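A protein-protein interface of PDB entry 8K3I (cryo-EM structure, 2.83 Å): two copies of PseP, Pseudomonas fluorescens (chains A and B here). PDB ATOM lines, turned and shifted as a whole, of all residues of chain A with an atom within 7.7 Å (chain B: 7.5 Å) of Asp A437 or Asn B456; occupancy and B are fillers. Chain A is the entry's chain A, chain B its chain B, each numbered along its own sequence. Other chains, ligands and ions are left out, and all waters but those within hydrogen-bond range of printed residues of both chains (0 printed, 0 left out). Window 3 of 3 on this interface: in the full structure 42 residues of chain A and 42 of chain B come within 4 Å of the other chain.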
ATOM      1  N   VAL A 434      30.680  23.943  -4.873  1.00  0.00           N
ATOM      2  CA  VAL A 434      31.289  22.623  -4.903  1.00  0.00           C
ATOM      3  C   VAL A 434      30.923  21.931  -6.208  1.00  0.00           C
ATOM      4  O   VAL A 434      29.785  22.022  -6.685  1.00  0.00           O
ATOM      5  CB  VAL A 434      30.840  21.797  -3.686  1.00  0.00           C
ATOM      6  CG1 VAL A 434      31.447  20.417  -3.729  1.00  0.00           C
ATOM      7  CG2 VAL A 434      31.224  22.498  -2.400  1.00  0.00           C
ATOM      8  N   ASP A 435      31.895  21.241  -6.801  1.00  0.00           N
ATOM      9  CA  ASP A 435      31.643  20.463  -8.006  1.00  0.00           C
ATOM     10  C   ASP A 435      30.669  19.333  -7.701  1.00  0.00           C
ATOM     11  O   ASP A 435      31.030  18.350  -7.050  1.00  0.00           O
ATOM     12  CB  ASP A 435      32.960  19.921  -8.565  1.00  0.00           C
ATOM     13  CG  ASP A 435      32.760  19.011  -9.757  1.00  0.00           C
ATOM     14  OD1 ASP A 435      32.426  19.515 -10.848  1.00  0.00           O
ATOM     15  OD2 ASP A 435      32.948  17.788  -9.603  1.00  0.00           O
ATOM     16  N   GLU A 436      29.426  19.469  -8.171  1.00  0.00           N
ATOM     17  CA  GLU A 436      28.369  18.524  -7.825  1.00  0.00           C
ATOM     18  C   GLU A 436      28.561  17.154  -8.457  1.00  0.00           C
ATOM     19  O   GLU A 436      27.852  16.218  -8.080  1.00  0.00           O
ATOM     20  CB  GLU A 436      27.001  19.091  -8.214  1.00  0.00           C
ATOM     21  CG  GLU A 436      26.781  19.254  -9.704  1.00  0.00           C
ATOM     22  CD  GLU A 436      27.122  20.644 -10.202  1.00  0.00           C
ATOM     23  OE1 GLU A 436      27.692  21.437  -9.424  1.00  0.00           O
ATOM     24  OE2 GLU A 436      26.830  20.941 -11.379  1.00  0.00           O
ATOM     25  N   ASP A 437      29.490  17.009  -9.401  1.00  0.00           N
ATOM     26  CA  ASP A 437      29.775  15.692  -9.959  1.00  0.00           C
ATOM     27  C   ASP A 437      30.636  14.862  -9.014  1.00  0.00           C
ATOM     28  O   ASP A 437      30.292  13.719  -8.693  1.00  0.00           O
ATOM     29  CB  ASP A 437      30.461  15.838 -11.317  1.00  0.00           C
ATOM     30  CG  ASP A 437      29.473  15.991 -12.451  1.00  0.00           C
ATOM     31  OD1 ASP A 437      28.486  15.229 -12.487  1.00  0.00           O
ATOM     32  OD2 ASP A 437      29.681  16.878 -13.304  1.00  0.00           O
ATOM     33  N   GLU A 438      31.762  15.416  -8.563  1.00  0.00           N
ATOM     34  CA  GLU A 438      32.644  14.679  -7.665  1.00  0.00           C
ATOM     35  C   GLU A 438      32.105  14.666  -6.240  1.00  0.00           C
ATOM     36  O   GLU A 438      32.161  13.639  -5.554  1.00  0.00           O
ATOM     37  CB  GLU A 438      34.052  15.274  -7.708  1.00  0.00           C
ATOM     38  N   TYR A 439      31.578  15.801  -5.770  1.00  0.00           N
ATOM     39  CA  TYR A 439      31.144  15.954  -4.379  1.00  0.00           C
ATOM     40  C   TYR A 439      29.702  16.450  -4.400  1.00  0.00           C
ATOM     41  O   TYR A 439      29.435  17.634  -4.186  1.00  0.00           O
ATOM     42  CB  TYR A 439      32.059  16.923  -3.631  1.00  0.00           C
ATOM     43  CG  TYR A 439      33.510  16.844  -4.044  1.00  0.00           C
ATOM     44  CD1 TYR A 439      34.272  15.718  -3.777  1.00  0.00           C
ATOM     45  CD2 TYR A 439      34.112  17.896  -4.720  1.00  0.00           C
ATOM     46  CE1 TYR A 439      35.591  15.645  -4.162  1.00  0.00           C
ATOM     47  CE2 TYR A 439      35.430  17.833  -5.110  1.00  0.00           C
ATOM     48  CZ  TYR A 439      36.165  16.706  -4.828  1.00  0.00           C
ATOM     49  OH  TYR A 439      37.481  16.639  -5.214  1.00  0.00           O
ATOM     50  N   GLY A 440      28.767  15.532  -4.619  1.00  0.00           N
ATOM     51  CA  GLY A 440      27.376  15.909  -4.749  1.00  0.00           C
ATOM     52  C   GLY A 440      26.524  15.520  -3.561  1.00  0.00           C
ATOM     53  O   GLY A 440      27.022  15.402  -2.439  1.00  0.00           O
ATOM     54  N   LEU A 441      25.234  15.324  -3.803  1.00  0.00           N
ATOM     55  CA  LEU A 441      24.327  14.911  -2.746  1.00  0.00           C
ATOM     56  C   LEU A 441      24.603  13.462  -2.353  1.00  0.00           C
ATOM     57  O   LEU A 441      24.803  12.611  -3.222  1.00  0.00           O
ATOM     58  CB  LEU A 441      22.879  15.065  -3.204  1.00  0.00           C
ATOM     59  CG  LEU A 441      21.795  15.081  -2.130  1.00  0.00           C
ATOM     60  CD1 LEU A 441      21.943  16.298  -1.239  1.00  0.00           C
ATOM     61  CD2 LEU A 441      20.425  15.045  -2.770  1.00  0.00           C
ATOM     62  N   PRO A 442      24.624  13.152  -1.060  1.00  0.00           N
ATOM     63  CA  PRO A 442      24.835  11.765  -0.636  1.00  0.00           C
ATOM     64  C   PRO A 442      23.678  10.873  -1.057  1.00  0.00           C
ATOM     65  O   PRO A 442      22.568  11.331  -1.333  1.00  0.00           O
ATOM     66  CB  PRO A 442      24.924  11.869   0.890  1.00  0.00           C
ATOM     67  CG  PRO A 442      25.249  13.302   1.156  1.00  0.00           C
ATOM     68  CD  PRO A 442      24.547  14.068   0.088  1.00  0.00           C
ATOM     69  N   LYS A 446      19.437  11.443  -1.931  1.00  0.00           N
ATOM     70  CA  LYS A 446      18.920  11.105  -3.252  1.00  0.00           C
ATOM     71  C   LYS A 446      17.823  10.058  -3.150  1.00  0.00           C
ATOM     72  O   LYS A 446      16.810  10.130  -3.856  1.00  0.00           O
ATOM     73  CB  LYS A 446      20.050  10.596  -4.145  1.00  0.00           C
ATOM     74  CG  LYS A 446      20.910  11.677  -4.751  1.00  0.00           C
ATOM     75  CD  LYS A 446      22.051  11.074  -5.545  1.00  0.00           C
ATOM     76  CE  LYS A 446      22.848  12.149  -6.256  1.00  0.00           C
ATOM     77  NZ  LYS A 446      23.254  11.721  -7.619  1.00  0.00           N
ATOM     78  N   SER A 632      25.820  21.020  -1.410  1.00  0.00           N
ATOM     79  CA  SER A 632      26.097  21.182  -2.839  1.00  0.00           C
ATOM     80  C   SER A 632      24.864  20.895  -3.696  1.00  0.00           C
ATOM     81  O   SER A 632      24.925  20.175  -4.694  1.00  0.00           O
ATOM     82  CB  SER A 632      27.281  20.313  -3.268  1.00  0.00           C
ATOM     83  OG  SER A 632      26.860  19.017  -3.637  1.00  0.00           O
ATOM     84  N   ARG A 796      36.766  21.658  -6.466  1.00  0.00           N
ATOM     85  CA  ARG A 796      36.601  21.192  -7.835  1.00  0.00           C
ATOM     86  C   ARG A 796      37.163  19.783  -7.962  1.00  0.00           C
ATOM     87  O   ARG A 796      37.689  19.211  -7.007  1.00  0.00           O
ATOM     88  CB  ARG A 796      37.289  22.137  -8.823  1.00  0.00           C
ATOM     89  CG  ARG A 796      37.264  23.600  -8.418  1.00  0.00           C
ATOM     90  CD  ARG A 796      35.852  24.148  -8.390  1.00  0.00           C
ATOM     91  NE  ARG A 796      35.102  23.794  -9.587  1.00  0.00           N
ATOM     92  CZ  ARG A 796      33.784  23.878  -9.693  1.00  0.00           C
ATOM     93  NH1 ARG A 796      33.036  24.296  -8.687  1.00  0.00           N
ATOM     94  NH2 ARG A 796      33.202  23.532 -10.838  1.00  0.00           N
ATOM     95  N   LYS A 797      37.044  19.222  -9.161  1.00  0.00           N
ATOM     96  CA  LYS A 797      37.718  17.967  -9.452  1.00  0.00           C
ATOM     97  C   LYS A 797      39.223  18.164  -9.342  1.00  0.00           C
ATOM     98  O   LYS A 797      39.752  19.241  -9.625  1.00  0.00           O
ATOM     99  CB  LYS A 797      37.348  17.467 -10.848  1.00  0.00           C
ATOM    100  N   ARG B 450      13.908  11.540 -12.117  1.00  0.00           N
ATOM    101  CA  ARG B 450      14.858  10.549 -11.618  1.00  0.00           C
ATOM    102  C   ARG B 450      16.189  10.636 -12.356  1.00  0.00           C
ATOM    103  O   ARG B 450      17.261  10.529 -11.746  1.00  0.00           O
ATOM    104  CB  ARG B 450      14.256   9.155 -11.759  1.00  0.00           C
ATOM    105  CG  ARG B 450      14.750   8.143 -10.761  1.00  0.00           C
ATOM    106  CD  ARG B 450      13.769   6.996 -10.632  1.00  0.00           C
ATOM    107  NE  ARG B 450      12.388   7.458 -10.575  1.00  0.00           N
ATOM    108  CZ  ARG B 450      11.397   6.956 -11.300  1.00  0.00           C
ATOM    109  NH1 ARG B 450      11.604   5.993 -12.183  1.00  0.00           N
ATOM    110  NH2 ARG B 450      10.166   7.430 -11.131  1.00  0.00           N
ATOM    111  N   PHE B 451      16.137  10.827 -13.674  1.00  0.00           N
ATOM    112  CA  PHE B 451      17.348  10.964 -14.474  1.00  0.00           C
ATOM    113  C   PHE B 451      18.128  12.217 -14.096  1.00  0.00           C
ATOM    114  O   PHE B 451      19.360  12.185 -14.007  1.00  0.00           O
ATOM    115  CB  PHE B 451      16.973  10.983 -15.954  1.00  0.00           C
ATOM    116  CG  PHE B 451      18.082  11.404 -16.866  1.00  0.00           C
ATOM    117  CD1 PHE B 451      19.098  10.529 -17.196  1.00  0.00           C
ATOM    118  CD2 PHE B 451      18.095  12.674 -17.413  1.00  0.00           C
ATOM    119  CE1 PHE B 451      20.109  10.914 -18.046  1.00  0.00           C
ATOM    120  CE2 PHE B 451      19.106  13.062 -18.265  1.00  0.00           C
ATOM    121  CZ  PHE B 451      20.111  12.183 -18.581  1.00  0.00           C
ATOM    122  N   ALA B 452      17.432  13.334 -13.890  1.00  0.00           N
ATOM    123  CA  ALA B 452      18.112  14.555 -13.476  1.00  0.00           C
ATOM    124  C   ALA B 452      18.761  14.376 -12.113  1.00  0.00           C
ATOM    125  O   ALA B 452      19.837  14.925 -11.850  1.00  0.00           O
ATOM    126  CB  ALA B 452      17.133  15.726 -13.456  1.00  0.00           C
ATOM    127  N   LEU B 453      18.113  13.617 -11.228  1.00  0.00           N
ATOM    128  CA  LEU B 453      18.718  13.310  -9.938  1.00  0.00           C
ATOM    129  C   LEU B 453      19.973  12.464 -10.103  1.00  0.00           C
ATOM    130  O   LEU B 453      20.976  12.688  -9.419  1.00  0.00           O
ATOM    131  CB  LEU B 453      17.700  12.603  -9.047  1.00  0.00           C
ATOM    132  CG  LEU B 453      18.058  12.444  -7.575  1.00  0.00           C
ATOM    133  CD1 LEU B 453      18.255  13.805  -6.952  1.00  0.00           C
ATOM    134  CD2 LEU B 453      16.970  11.676  -6.855  1.00  0.00           C
ATOM    135  N   ALA B 454      19.939  11.486 -11.012  1.00  0.00           N
ATOM    136  CA  ALA B 454      21.089  10.605 -11.198  1.00  0.00           C
ATOM    137  C   ALA B 454      22.260  11.318 -11.862  1.00  0.00           C
ATOM    138  O   ALA B 454      23.409  10.900 -11.696  1.00  0.00           O
ATOM    139  CB  ALA B 454      20.691   9.385 -12.022  1.00  0.00           C
ATOM    140  N   ARG B 455      21.995  12.374 -12.619  1.00  0.00           N
ATOM    141  CA  ARG B 455      23.029  13.101 -13.339  1.00  0.00           C
ATOM    142  C   ARG B 455      23.573  14.288 -12.562  1.00  0.00           C
ATOM    143  O   ARG B 455      24.381  15.045 -13.108  1.00  0.00           O
ATOM    144  CB  ARG B 455      22.490  13.580 -14.687  1.00  0.00           C
ATOM    145  CG  ARG B 455      22.367  12.488 -15.721  1.00  0.00           C
ATOM    146  CD  ARG B 455      23.725  11.942 -16.104  1.00  0.00           C
ATOM    147  NE  ARG B 455      24.174  12.494 -17.375  1.00  0.00           N
ATOM    148  CZ  ARG B 455      23.961  11.924 -18.552  1.00  0.00           C
ATOM    149  NH1 ARG B 455      23.339  10.762 -18.653  1.00  0.00           N
ATOM    150  NH2 ARG B 455      24.377  12.539 -19.654  1.00  0.00           N
ATOM    151  N   ASN B 456      23.151  14.466 -11.310  1.00  0.00           N
ATOM    152  CA  ASN B 456      23.560  15.600 -10.483  1.00  0.00           C
ATOM    153  C   ASN B 456      23.205  16.926 -11.148  1.00  0.00           C
ATOM    154  O   ASN B 456      23.947  17.904 -11.062  1.00  0.00           O
ATOM    155  CB  ASN B 456      25.050  15.537 -10.145  1.00  0.00           C
ATOM    156  CG  ASN B 456      25.477  14.169  -9.652  1.00  0.00           C
ATOM    157  OD1 ASN B 456      24.958  13.668  -8.660  1.00  0.00           O
ATOM    158  ND2 ASN B 456      26.428  13.559 -10.345  1.00  0.00           N
ATOM    159  N   PHE B 457      22.048  16.961 -11.807  1.00  0.00           N
ATOM    160  CA  PHE B 457      21.587  18.162 -12.491  1.00  0.00           C
ATOM    161  C   PHE B 457      20.939  19.128 -11.511  1.00  0.00           C
ATOM    162  O   PHE B 457      19.787  19.528 -11.693  1.00  0.00           O
ATOM    163  CB  PHE B 457      20.600  17.809 -13.602  1.00  0.00           C
ATOM    164  CG  PHE B 457      21.250  17.302 -14.850  1.00  0.00           C
ATOM    165  CD1 PHE B 457      22.615  17.414 -15.032  1.00  0.00           C
ATOM    166  CD2 PHE B 457      20.495  16.711 -15.845  1.00  0.00           C
ATOM    167  CE1 PHE B 457      23.212  16.946 -16.181  1.00  0.00           C
ATOM    168  CE2 PHE B 457      21.087  16.245 -16.995  1.00  0.00           C
ATOM    169  CZ  PHE B 457      22.446  16.362 -17.163  1.00  0.00           C
ATOM    170  N   TYR B 458      21.673  19.500 -10.467  1.00  0.00           N
ATOM    171  CA  TYR B 458      21.221  20.479  -9.489  1.00  0.00           C
ATOM    172  C   TYR B 458      22.307  21.495  -9.159  1.00  0.00           C
ATOM    173  O   TYR B 458      22.442  21.912  -8.006  1.00  0.00           O
ATOM    174  CB  TYR B 458      20.703  19.797  -8.219  1.00  0.00           C
ATOM    175  CG  TYR B 458      21.596  18.704  -7.689  1.00  0.00           C
ATOM    176  CD1 TYR B 458      21.302  17.375  -7.952  1.00  0.00           C
ATOM    177  CD2 TYR B 458      22.766  18.989  -7.009  1.00  0.00           C
ATOM    178  CE1 TYR B 458      22.107  16.362  -7.491  1.00  0.00           C
ATOM    179  CE2 TYR B 458      23.591  17.975  -6.556  1.00  0.00           C
ATOM    180  CZ  TYR B 458      23.255  16.666  -6.803  1.00  0.00           C
ATOM    181  OH  TYR B 458      24.064  15.652  -6.357  1.00  0.00           O
ATOM    182  N   GLY B 459      23.080  21.908 -10.158  1.00  0.00           N
ATOM    183  CA  GLY B 459      23.990  23.018 -10.005  1.00  0.00           C
ATOM    184  C   GLY B 459      23.283  24.342 -10.197  1.00  0.00           C
ATOM    185  O   GLY B 459      22.064  24.420 -10.331  1.00  0.00           O
ATOM    186  N   SER B 664      17.197  24.291 -11.374  1.00  0.00           N
ATOM    187  CA  SER B 664      17.752  23.584 -12.520  1.00  0.00           C
ATOM    188  C   SER B 664      17.288  22.138 -12.541  1.00  0.00           C
ATOM    189  O   SER B 664      17.172  21.535 -13.613  1.00  0.00           O
ATOM    190  CB  SER B 664      19.277  23.655 -12.493  1.00  0.00           C
ATOM    191  OG  SER B 664      19.801  22.918 -11.404  1.00  0.00           O
ATOM    192  N   PHE B 665      16.968  21.595 -11.367  1.00  0.00           N
ATOM    193  CA  PHE B 665      16.653  20.183 -11.217  1.00  0.00           C
ATOM    194  C   PHE B 665      15.442  19.761 -12.041  1.00  0.00           C
ATOM    195  O   PHE B 665      15.277  18.568 -12.311  1.00  0.00           O
ATOM    196  CB  PHE B 665      16.444  19.892  -9.728  1.00  0.00           C
ATOM    197  CG  PHE B 665      15.944  18.514  -9.432  1.00  0.00           C
ATOM    198  CD1 PHE B 665      16.798  17.430  -9.480  1.00  0.00           C
ATOM    199  CD2 PHE B 665      14.628  18.307  -9.066  1.00  0.00           C
ATOM    200  CE1 PHE B 665      16.344  16.162  -9.196  1.00  0.00           C
ATOM    201  CE2 PHE B 665      14.168  17.047  -8.779  1.00  0.00           C
ATOM    202  CZ  PHE B 665      15.027  15.970  -8.843  1.00  0.00           C
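Among the printed residues, merely in contact across the chains: Ser A632 with Tyr B458 (3.2 Å), Glu A436 with Asn B456 (3.4 Å), Gly A440 with Tyr B458 (3.7 Å), Lys A446 with Tyr B458 (3.7 Å), Glu A436 with Gly B459 (3.8 Å) and Glu A436 with Tyr B458 (3.95 Å).
The backbone carbonyl oxygen of Leu B453 sits at hydrogen-bond distance from the side-chain amino group of Lys A446, at 3.1 Å.
The side-chain carboxylate (OD1) of Asp A437 is in hydrogen-bond range of the side-chain amide nitrogen (ND2) of Asn B456 (3.4 Å).
The backbone NH (N) of Leu A441 lies within hydrogen-bond range of the side-chain hydroxyl (OH) of Tyr B458 (2.8 Å).
The side-chain amino group (NZ) of Lys A446 lies within hydrogen-bond range of the side-chain amide oxygen (OD1) of Asn B456.
Of chain B, only Asn B456 (3.4 Å) comes within 4 Å of Asp A437.
Asn B456 touches three residues of chain A.
Printed residues of chain B within 4 Å of Leu A441: Tyr B458.
Of the printed residues of chain B, Gly A440 touches Tyr B458.
The nearest residue of chain B that does not touch Asp A437 is Arg B455 (4.2 Å).
The nearest printed residue of chain A that does not touch Asn B456 is Gly A440 (5.1 Å).
The nearest printed residue of chain A that does not touch Leu B453 is Leu A441 (4.9 Å).
Hydrophobic or aromatic side chains of chain A that line the printed part of chain B: Leu A441.
Of the 12 printed residues of chain B, 4 touch a printed residue of chain A.
Among the printed residues, 10 pairs touch across the chains.
Among the printed residues, no Asp or Glu carboxylate lies within 4 Å of a Lys or Arg side-chain nitrogen of the other chain.
The side-chain amide oxygen (OD1) of Asn B456 sits at hydrogen-bond distance from the side-chain hydroxyl (OH) of Tyr B458, 3.2 Å away.
The backbone carbonyl oxygen of Gly B459 is in hydrogen-bond range of the side-chain hydroxyl of Ser B664, 2.9 Å away.
O of Tyr A439 sits at hydrogen-bond distance from OG of Ser A632 (3.0 Å).
No position is printed for both chains.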
